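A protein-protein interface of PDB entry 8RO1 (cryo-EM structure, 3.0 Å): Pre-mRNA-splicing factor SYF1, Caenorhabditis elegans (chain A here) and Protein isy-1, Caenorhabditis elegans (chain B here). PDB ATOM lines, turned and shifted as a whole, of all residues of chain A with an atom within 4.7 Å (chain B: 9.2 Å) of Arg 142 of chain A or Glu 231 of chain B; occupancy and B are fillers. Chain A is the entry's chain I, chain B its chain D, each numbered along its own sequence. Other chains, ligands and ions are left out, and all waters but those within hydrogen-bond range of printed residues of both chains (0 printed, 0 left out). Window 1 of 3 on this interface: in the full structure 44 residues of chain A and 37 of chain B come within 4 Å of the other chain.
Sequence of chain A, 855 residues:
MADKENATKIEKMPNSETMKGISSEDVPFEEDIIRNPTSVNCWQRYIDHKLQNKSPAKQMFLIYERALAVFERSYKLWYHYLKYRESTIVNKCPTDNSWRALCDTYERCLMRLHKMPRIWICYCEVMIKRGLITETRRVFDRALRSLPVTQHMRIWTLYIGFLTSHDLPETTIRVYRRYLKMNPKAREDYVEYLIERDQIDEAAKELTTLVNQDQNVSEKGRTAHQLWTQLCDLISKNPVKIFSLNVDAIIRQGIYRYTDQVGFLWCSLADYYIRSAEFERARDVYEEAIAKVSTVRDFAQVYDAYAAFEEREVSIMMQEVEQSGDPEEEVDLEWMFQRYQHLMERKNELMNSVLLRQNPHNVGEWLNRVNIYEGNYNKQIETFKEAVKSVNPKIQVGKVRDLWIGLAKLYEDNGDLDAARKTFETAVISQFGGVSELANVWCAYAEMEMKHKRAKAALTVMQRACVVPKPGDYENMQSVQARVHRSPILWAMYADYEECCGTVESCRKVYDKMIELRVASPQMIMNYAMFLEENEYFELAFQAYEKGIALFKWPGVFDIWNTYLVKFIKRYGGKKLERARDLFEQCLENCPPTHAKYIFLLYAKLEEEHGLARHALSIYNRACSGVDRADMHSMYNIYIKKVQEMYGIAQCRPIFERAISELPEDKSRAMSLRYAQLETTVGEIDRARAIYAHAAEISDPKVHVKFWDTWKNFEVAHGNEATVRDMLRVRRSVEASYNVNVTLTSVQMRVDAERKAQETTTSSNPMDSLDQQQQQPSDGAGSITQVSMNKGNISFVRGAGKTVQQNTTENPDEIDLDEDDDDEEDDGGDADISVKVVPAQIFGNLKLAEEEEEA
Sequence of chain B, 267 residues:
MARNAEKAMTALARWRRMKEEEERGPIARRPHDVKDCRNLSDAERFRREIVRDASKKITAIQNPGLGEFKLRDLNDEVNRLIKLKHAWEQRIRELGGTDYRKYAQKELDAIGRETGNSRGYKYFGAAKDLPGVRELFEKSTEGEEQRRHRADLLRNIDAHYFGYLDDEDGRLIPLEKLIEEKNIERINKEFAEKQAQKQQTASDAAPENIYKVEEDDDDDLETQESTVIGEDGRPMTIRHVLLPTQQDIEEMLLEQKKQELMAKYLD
Hydrophobic or aromatic side chains of chain B within 4 Å of the printed part of chain A: Phe 162, Tyr 164 and Met 236.
Of the 11 printed residues of chain A, 6 touch a printed residue of chain B.
Among the printed residues, Asp or Glu carboxylates within 4 Å of a Lys or Arg side-chain nitrogen of the other chain: Arg 142 of chain A with Asp 232 of chain B (2.9 Å).
NH2 of Arg 234 of chain B is in salt-bridge range of OD2 of Asp 232 of chain B (2.6 Å).
OE2 of Glu 107 of chain A is in salt-bridge range of NH2 of Arg 142 of chain A, 3.0 Å away.
N of Met 236 of chain B is in hydrogen-bond range of O of Val 228 of chain B.
The guanidinium group (NE) of Arg 234 of chain B lies close to the guanidinium group (NE) of Arg 138 of chain A (3.4 Å).
The side-chain carboxylate (OD1) of Asp 232 of chain B is in salt-bridge range of the guanidinium group (NH1) of Arg 142 of chain A (2.9 Å).
O of Gly 163 of chain B is in hydrogen-bond range of NH1 of Arg 145 of chain A, 3.2 Å away.
O of Phe 162 of chain B lies within hydrogen-bond range of NE of Arg 145 of chain A (3.1 Å).
Glu 107 of chain A touches Met 236 of chain B.
Glu 231 of chain B touches Trp 120 of chain A (OE2 to CH2, 3.9 Å).
OE2 of Glu 231 of chain B touches CD of Arg 142 of chain A (3.9 Å).
O of Leu 144 of chain A touches CE1 of Phe 162 of chain B (3.7 Å).
Arg 145 of chain A touches Tyr 164 of chain B (NH1 to CD1, 3.4 Å).
Of the printed residues of chain B, Trp 120 of chain A touches Glu 231 (3.9 Å).
Of the printed residues of chain B, Arg 142 of chain A touches Glu 231 and Asp 232.
Of the printed residues of chain A, Phe 162 of chain B touches Leu 144 and Arg 145.
Printed residues of chain A within 4 Å of Glu 231 of chain B: Trp 120 (3.9 Å) and Arg 142 (3.9 Å).
Printed residues of chain A within 4 Å of Met 236 of chain B: Glu 107 (3.7 Å).
The nearest residue of chain A that does not touch Glu 231 of chain B is Arg 145 of chain A (4.5 Å).
The nearest printed residue of chain B that does not touch Trp 120 of chain A is Asp 232 of chain B (8.9 Å).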
ATOM      1  N   GLU A 107      23.704 -17.919  -5.602  1.00  0.00           N
ATOM      2  CA  GLU A 107      23.040 -16.621  -5.678  1.00  0.00           C
ATOM      3  C   GLU A 107      23.990 -15.486  -5.338  1.00  0.00           C
ATOM      4  O   GLU A 107      24.007 -14.454  -6.011  1.00  0.00           O
ATOM      5  CB  GLU A 107      21.836 -16.590  -4.749  1.00  0.00           C
ATOM      6  CG  GLU A 107      20.727 -17.549  -5.101  1.00  0.00           C
ATOM      7  CD  GLU A 107      20.024 -17.194  -6.395  1.00  0.00           C
ATOM      8  OE1 GLU A 107      20.272 -16.099  -6.938  1.00  0.00           O
ATOM      9  OE2 GLU A 107      19.205 -18.004  -6.868  1.00  0.00           O
ATOM     10  N   TRP A 120      26.169 -19.992 -14.232  1.00  0.00           N
ATOM     11  CA  TRP A 120      24.762 -20.314 -14.436  1.00  0.00           C
ATOM     12  C   TRP A 120      24.562 -21.786 -14.745  1.00  0.00           C
ATOM     13  O   TRP A 120      23.617 -22.405 -14.253  1.00  0.00           O
ATOM     14  CB  TRP A 120      24.185 -19.461 -15.552  1.00  0.00           C
ATOM     15  CG  TRP A 120      23.818 -18.071 -15.164  1.00  0.00           C
ATOM     16  CD1 TRP A 120      24.409 -16.925 -15.563  1.00  0.00           C
ATOM     17  CD2 TRP A 120      22.733 -17.694 -14.324  1.00  0.00           C
ATOM     18  NE1 TRP A 120      23.763 -15.844 -15.020  1.00  0.00           N
ATOM     19  CE2 TRP A 120      22.728 -16.300 -14.253  1.00  0.00           C
ATOM     20  CE3 TRP A 120      21.761 -18.406 -13.621  1.00  0.00           C
ATOM     21  CZ2 TRP A 120      21.796 -15.608 -13.511  1.00  0.00           C
ATOM     22  CZ3 TRP A 120      20.842 -17.715 -12.893  1.00  0.00           C
ATOM     23  CH2 TRP A 120      20.864 -16.333 -12.842  1.00  0.00           C
ATOM     24  N   ARG A 138      12.875 -21.844 -12.940  1.00  0.00           N
ATOM     25  CA  ARG A 138      13.007 -20.407 -12.720  1.00  0.00           C
ATOM     26  C   ARG A 138      14.460 -19.950 -12.750  1.00  0.00           C
ATOM     27  O   ARG A 138      14.755 -18.852 -13.227  1.00  0.00           O
ATOM     28  CB  ARG A 138      12.333 -20.031 -11.407  1.00  0.00           C
ATOM     29  CG  ARG A 138      10.859 -20.397 -11.361  1.00  0.00           C
ATOM     30  CD  ARG A 138      10.240 -20.069 -10.031  1.00  0.00           C
ATOM     31  NE  ARG A 138       8.857 -20.526  -9.946  1.00  0.00           N
ATOM     32  CZ  ARG A 138       8.160 -20.653  -8.821  1.00  0.00           C
ATOM     33  NH1 ARG A 138       6.907 -21.093  -8.885  1.00  0.00           N
ATOM     34  NH2 ARG A 138       8.678 -20.353  -7.639  1.00  0.00           N
ATOM     35  N   VAL A 139      15.370 -20.745 -12.195  1.00  0.00           N
ATOM     36  CA  VAL A 139      16.796 -20.453 -12.310  1.00  0.00           C
ATOM     37  C   VAL A 139      17.211 -20.397 -13.773  1.00  0.00           C
ATOM     38  O   VAL A 139      18.007 -19.544 -14.179  1.00  0.00           O
ATOM     39  CB  VAL A 139      17.616 -21.501 -11.537  1.00  0.00           C
ATOM     40  CG1 VAL A 139      19.111 -21.351 -11.801  1.00  0.00           C
ATOM     41  CG2 VAL A 139      17.306 -21.448 -10.047  1.00  0.00           C
ATOM     42  N   PHE A 140      16.694 -21.325 -14.583  1.00  0.00           N
ATOM     43  CA  PHE A 140      16.927 -21.313 -16.026  1.00  0.00           C
ATOM     44  C   PHE A 140      16.392 -20.060 -16.696  1.00  0.00           C
ATOM     45  O   PHE A 140      17.039 -19.499 -17.586  1.00  0.00           O
ATOM     46  CB  PHE A 140      16.267 -22.539 -16.659  1.00  0.00           C
ATOM     47  CG  PHE A 140      17.101 -23.778 -16.636  1.00  0.00           C
ATOM     48  CD1 PHE A 140      18.248 -23.877 -17.384  1.00  0.00           C
ATOM     49  CD2 PHE A 140      16.716 -24.855 -15.877  1.00  0.00           C
ATOM     50  CE1 PHE A 140      18.998 -25.010 -17.356  1.00  0.00           C
ATOM     51  CE2 PHE A 140      17.459 -25.991 -15.849  1.00  0.00           C
ATOM     52  CZ  PHE A 140      18.594 -26.080 -16.595  1.00  0.00           C
ATOM     53  N   ASP A 141      15.179 -19.653 -16.346  1.00  0.00           N
ATOM     54  CA  ASP A 141      14.615 -18.435 -16.913  1.00  0.00           C
ATOM     55  C   ASP A 141      15.451 -17.203 -16.568  1.00  0.00           C
ATOM     56  O   ASP A 141      15.578 -16.287 -17.386  1.00  0.00           O
ATOM     57  CB  ASP A 141      13.175 -18.263 -16.438  1.00  0.00           C
ATOM     58  CG  ASP A 141      12.199 -19.201 -17.143  1.00  0.00           C
ATOM     59  OD1 ASP A 141      12.529 -19.759 -18.212  1.00  0.00           O
ATOM     60  OD2 ASP A 141      11.080 -19.383 -16.624  1.00  0.00           O
ATOM     61  N   ARG A 142      16.023 -17.157 -15.363  1.00  0.00           N
ATOM     62  CA  ARG A 142      16.948 -16.081 -15.014  1.00  0.00           C
ATOM     63  C   ARG A 142      18.207 -16.104 -15.865  1.00  0.00           C
ATOM     64  O   ARG A 142      18.684 -15.053 -16.300  1.00  0.00           O
ATOM     65  CB  ARG A 142      17.348 -16.187 -13.551  1.00  0.00           C
ATOM     66  CG  ARG A 142      16.259 -15.911 -12.563  1.00  0.00           C
ATOM     67  CD  ARG A 142      16.744 -16.199 -11.157  1.00  0.00           C
ATOM     68  NE  ARG A 142      15.638 -16.172 -10.212  1.00  0.00           N
ATOM     69  CZ  ARG A 142      15.658 -16.696  -8.993  1.00  0.00           C
ATOM     70  NH1 ARG A 142      14.553 -16.650  -8.253  1.00  0.00           N
ATOM     71  NH2 ARG A 142      16.748 -17.255  -8.489  1.00  0.00           N
ATOM     72  N   ALA A 143      18.775 -17.288 -16.086  1.00  0.00           N
ATOM     73  CA  ALA A 143      19.984 -17.409 -16.893  1.00  0.00           C
ATOM     74  C   ALA A 143      19.785 -16.894 -18.305  1.00  0.00           C
ATOM     75  O   ALA A 143      20.710 -16.347 -18.906  1.00  0.00           O
ATOM     76  CB  ALA A 143      20.439 -18.861 -16.947  1.00  0.00           C
ATOM     77  N   LEU A 144      18.605 -17.106 -18.871  1.00  0.00           N
ATOM     78  CA  LEU A 144      18.319 -16.584 -20.201  1.00  0.00           C
ATOM     79  C   LEU A 144      18.206 -15.064 -20.213  1.00  0.00           C
ATOM     80  O   LEU A 144      18.709 -14.407 -21.130  1.00  0.00           O
ATOM     81  CB  LEU A 144      17.034 -17.216 -20.715  1.00  0.00           C
ATOM     82  CG  LEU A 144      17.105 -18.724 -20.942  1.00  0.00           C
ATOM     83  CD1 LEU A 144      15.728 -19.226 -21.240  1.00  0.00           C
ATOM     84  CD2 LEU A 144      18.053 -19.107 -22.045  1.00  0.00           C
ATOM     85  N   ARG A 145      17.543 -14.487 -19.214  1.00  0.00           N
ATOM     86  CA  ARG A 145      17.468 -13.033 -19.114  1.00  0.00           C
ATOM     87  C   ARG A 145      18.819 -12.399 -18.833  1.00  0.00           C
ATOM     88  O   ARG A 145      19.069 -11.271 -19.266  1.00  0.00           O
ATOM     89  CB  ARG A 145      16.472 -12.624 -18.040  1.00  0.00           C
ATOM     90  CG  ARG A 145      15.044 -12.888 -18.415  1.00  0.00           C
ATOM     91  CD  ARG A 145      14.097 -12.357 -17.381  1.00  0.00           C
ATOM     92  NE  ARG A 145      12.716 -12.691 -17.699  1.00  0.00           N
ATOM     93  CZ  ARG A 145      11.663 -12.360 -16.964  1.00  0.00           C
ATOM     94  NH1 ARG A 145      10.458 -12.778 -17.337  1.00  0.00           N
ATOM     95  NH2 ARG A 145      11.775 -11.616 -15.874  1.00  0.00           N
ATOM     96  N   SER A 146      19.703 -13.099 -18.136  1.00  0.00           N
ATOM     97  CA  SER A 146      20.948 -12.513 -17.663  1.00  0.00           C
ATOM     98  C   SER A 146      22.098 -12.623 -18.651  1.00  0.00           C
ATOM     99  O   SER A 146      22.876 -11.677 -18.782  1.00  0.00           O
ATOM    100  CB  SER A 146      21.349 -13.192 -16.360  1.00  0.00           C
ATOM    101  OG  SER A 146      22.394 -12.489 -15.731  1.00  0.00           O
ATOM    102  N   PHE B 162      11.888 -14.176 -23.823  1.00  0.00           N
ATOM    103  CA  PHE B 162      12.352 -13.975 -22.455  1.00  0.00           C
ATOM    104  C   PHE B 162      11.333 -14.360 -21.389  1.00  0.00           C
ATOM    105  O   PHE B 162      11.609 -14.143 -20.206  1.00  0.00           O
ATOM    106  CB  PHE B 162      12.807 -12.526 -22.279  1.00  0.00           C
ATOM    107  CG  PHE B 162      14.080 -12.214 -23.014  1.00  0.00           C
ATOM    108  CD1 PHE B 162      15.282 -12.720 -22.588  1.00  0.00           C
ATOM    109  CD2 PHE B 162      14.065 -11.412 -24.129  1.00  0.00           C
ATOM    110  CE1 PHE B 162      16.440 -12.444 -23.264  1.00  0.00           C
ATOM    111  CE2 PHE B 162      15.220 -11.131 -24.805  1.00  0.00           C
ATOM    112  CZ  PHE B 162      16.412 -11.648 -24.372  1.00  0.00           C
ATOM    113  N   GLY B 163      10.182 -14.924 -21.743  1.00  0.00           N
ATOM    114  CA  GLY B 163       9.295 -15.444 -20.723  1.00  0.00           C
ATOM    115  C   GLY B 163       8.550 -14.410 -19.923  1.00  0.00           C
ATOM    116  O   GLY B 163       8.257 -14.643 -18.749  1.00  0.00           O
ATOM    117  N   TYR B 164       8.228 -13.273 -20.528  1.00  0.00           N
ATOM    118  CA  TYR B 164       7.316 -12.329 -19.904  1.00  0.00           C
ATOM    119  C   TYR B 164       5.859 -12.748 -20.061  1.00  0.00           C
ATOM    120  O   TYR B 164       5.013 -12.274 -19.296  1.00  0.00           O
ATOM    121  CB  TYR B 164       7.523 -10.930 -20.485  1.00  0.00           C
ATOM    122  CG  TYR B 164       8.881 -10.350 -20.175  1.00  0.00           C
ATOM    123  CD1 TYR B 164       9.221  -9.991 -18.885  1.00  0.00           C
ATOM    124  CD2 TYR B 164       9.818 -10.154 -21.169  1.00  0.00           C
ATOM    125  CE1 TYR B 164      10.453  -9.473 -18.594  1.00  0.00           C
ATOM    126  CE2 TYR B 164      11.052  -9.629 -20.883  1.00  0.00           C
ATOM    127  CZ  TYR B 164      11.361  -9.288 -19.593  1.00  0.00           C
ATOM    128  OH  TYR B 164      12.593  -8.766 -19.292  1.00  0.00           O
ATOM    129  N   VAL B 228      13.930 -10.740   0.087  1.00  0.00           N
ATOM    130  CA  VAL B 228      13.829  -9.677  -0.906  1.00  0.00           C
ATOM    131  C   VAL B 228      13.054 -10.213  -2.101  1.00  0.00           C
ATOM    132  O   VAL B 228      12.952 -11.421  -2.315  1.00  0.00           O
ATOM    133  CB  VAL B 228      15.209  -9.148  -1.371  1.00  0.00           C
ATOM    134  CG1 VAL B 228      16.022  -8.639  -0.200  1.00  0.00           C
ATOM    135  CG2 VAL B 228      15.982 -10.210  -2.138  1.00  0.00           C
ATOM    136  N   ILE B 229      12.496  -9.289  -2.878  1.00  0.00           N
ATOM    137  CA  ILE B 229      11.914  -9.629  -4.173  1.00  0.00           C
ATOM    138  C   ILE B 229      13.041  -9.988  -5.132  1.00  0.00           C
ATOM    139  O   ILE B 229      13.946  -9.183  -5.380  1.00  0.00           O
ATOM    140  CB  ILE B 229      11.056  -8.477  -4.712  1.00  0.00           C
ATOM    141  CG1 ILE B 229       9.959  -8.078  -3.710  1.00  0.00           C
ATOM    142  CG2 ILE B 229      10.442  -8.842  -6.067  1.00  0.00           C
ATOM    143  CD1 ILE B 229       9.016  -9.207  -3.280  1.00  0.00           C
ATOM    144  N   GLY B 230      12.979 -11.191  -5.687  1.00  0.00           N
ATOM    145  CA  GLY B 230      14.016 -11.701  -6.554  1.00  0.00           C
ATOM    146  C   GLY B 230      13.924 -11.177  -7.974  1.00  0.00           C
ATOM    147  O   GLY B 230      13.134 -10.292  -8.307  1.00  0.00           O
ATOM    148  N   GLU B 231      14.792 -11.741  -8.820  1.00  0.00           N
ATOM    149  CA  GLU B 231      14.908 -11.311 -10.212  1.00  0.00           C
ATOM    150  C   GLU B 231      13.602 -11.480 -10.974  1.00  0.00           C
ATOM    151  O   GLU B 231      13.229 -10.614 -11.773  1.00  0.00           O
ATOM    152  CB  GLU B 231      15.984 -12.126 -10.921  1.00  0.00           C
ATOM    153  CG  GLU B 231      17.407 -11.875 -10.491  1.00  0.00           C
ATOM    154  CD  GLU B 231      18.405 -12.390 -11.513  1.00  0.00           C
ATOM    155  OE1 GLU B 231      18.301 -12.023 -12.702  1.00  0.00           O
ATOM    156  OE2 GLU B 231      19.281 -13.190 -11.127  1.00  0.00           O
ATOM    157  N   ASP B 232      12.891 -12.582 -10.734  1.00  0.00           N
ATOM    158  CA  ASP B 232      11.664 -12.900 -11.455  1.00  0.00           C
ATOM    159  C   ASP B 232      10.403 -12.456 -10.722  1.00  0.00           C
ATOM    160  O   ASP B 232       9.318 -12.976 -11.002  1.00  0.00           O
ATOM    161  CB  ASP B 232      11.606 -14.404 -11.754  1.00  0.00           C
ATOM    162  CG  ASP B 232      11.663 -15.264 -10.503  1.00  0.00           C
ATOM    163  OD1 ASP B 232      12.638 -15.129  -9.735  1.00  0.00           O
ATOM    164  OD2 ASP B 232      10.737 -16.072 -10.292  1.00  0.00           O
ATOM    165  N   GLY B 233      10.512 -11.510  -9.794  1.00  0.00           N
ATOM    166  CA  GLY B 233       9.352 -11.048  -9.061  1.00  0.00           C
ATOM    167  C   GLY B 233       8.874 -11.926  -7.928  1.00  0.00           C
ATOM    168  O   GLY B 233       7.929 -11.532  -7.231  1.00  0.00           O
ATOM    169  N   ARG B 234       9.498 -13.081  -7.699  1.00  0.00           N
ATOM    170  CA  ARG B 234       9.075 -14.012  -6.659  1.00  0.00           C
ATOM    171  C   ARG B 234      10.000 -13.903  -5.451  1.00  0.00           C
ATOM    172  O   ARG B 234      11.208 -13.720  -5.622  1.00  0.00           O
ATOM    173  CB  ARG B 234       9.082 -15.457  -7.159  1.00  0.00           C
ATOM    174  CG  ARG B 234       8.126 -15.744  -8.308  1.00  0.00           C
ATOM    175  CD  ARG B 234       8.104 -17.236  -8.602  1.00  0.00           C
ATOM    176  NE  ARG B 234       7.220 -17.605  -9.706  1.00  0.00           N
ATOM    177  CZ  ARG B 234       7.544 -17.593 -10.994  1.00  0.00           C
ATOM    178  NH1 ARG B 234       6.625 -17.938 -11.893  1.00  0.00           N
ATOM    179  NH2 ARG B 234       8.761 -17.277 -11.408  1.00  0.00           N
ATOM    180  N   PRO B 235       9.543 -14.004  -4.197  1.00  0.00           N
ATOM    181  CA  PRO B 235      10.421 -13.622  -3.084  1.00  0.00           C
ATOM    182  C   PRO B 235      11.452 -14.704  -2.807  1.00  0.00           C
ATOM    183  O   PRO B 235      11.126 -15.892  -2.761  1.00  0.00           O
ATOM    184  CB  PRO B 235       9.457 -13.474  -1.900  1.00  0.00           C
ATOM    185  CG  PRO B 235       8.116 -13.416  -2.481  1.00  0.00           C
ATOM    186  CD  PRO B 235       8.177 -14.257  -3.701  1.00  0.00           C
ATOM    187  N   MET B 236      12.698 -14.278  -2.622  1.00  0.00           N
ATOM    188  CA  MET B 236      13.831 -15.145  -2.337  1.00  0.00           C
ATOM    189  C   MET B 236      14.425 -14.743  -0.996  1.00  0.00           C
ATOM    190  O   MET B 236      13.959 -13.804  -0.347  1.00  0.00           O
ATOM    191  CB  MET B 236      14.869 -15.080  -3.463  1.00  0.00           C
ATOM    192  CG  MET B 236      15.625 -13.764  -3.630  1.00  0.00           C
ATOM    193  SD  MET B 236      16.871 -13.865  -4.937  1.00  0.00           S
ATOM    194  CE  MET B 236      18.110 -14.927  -4.204  1.00  0.00           C
ATOM    195  N   THR B 237      15.454 -15.475  -0.583  1.00  0.00           N
ATOM    196  CA  THR B 237      16.226 -15.152   0.605  1.00  0.00           C
ATOM    197  C   THR B 237      17.712 -15.214   0.297  1.00  0.00           C
ATOM    198  O   THR B 237      18.159 -16.078  -0.461  1.00  0.00           O
ATOM    199  CB  THR B 237      15.874 -16.105   1.762  1.00  0.00           C
ATOM    200  OG1 THR B 237      16.639 -15.764   2.920  1.00  0.00           O
ATOM    201  CG2 THR B 237      16.124 -17.576   1.395  1.00  0.00           C
ATOM    202  N   ILE B 238      18.467 -14.296   0.892  1.00  0.00           N
ATOM    203  CA  ILE B 238      19.921 -14.268   0.798  1.00  0.00           C
ATOM    204  C   ILE B 238      20.462 -14.582   2.176  1.00  0.00           C
ATOM    205  O   ILE B 238      20.070 -13.943   3.154  1.00  0.00           O
ATOM    206  CB  ILE B 238      20.440 -12.901   0.311  1.00  0.00           C
ATOM    207  CG1 ILE B 238      19.958 -12.597  -1.107  1.00  0.00           C
ATOM    208  CG2 ILE B 238      21.993 -12.844   0.334  1.00  0.00           C
ATOM    209  CD1 ILE B 238      18.619 -11.950  -1.235  1.00  0.00           C
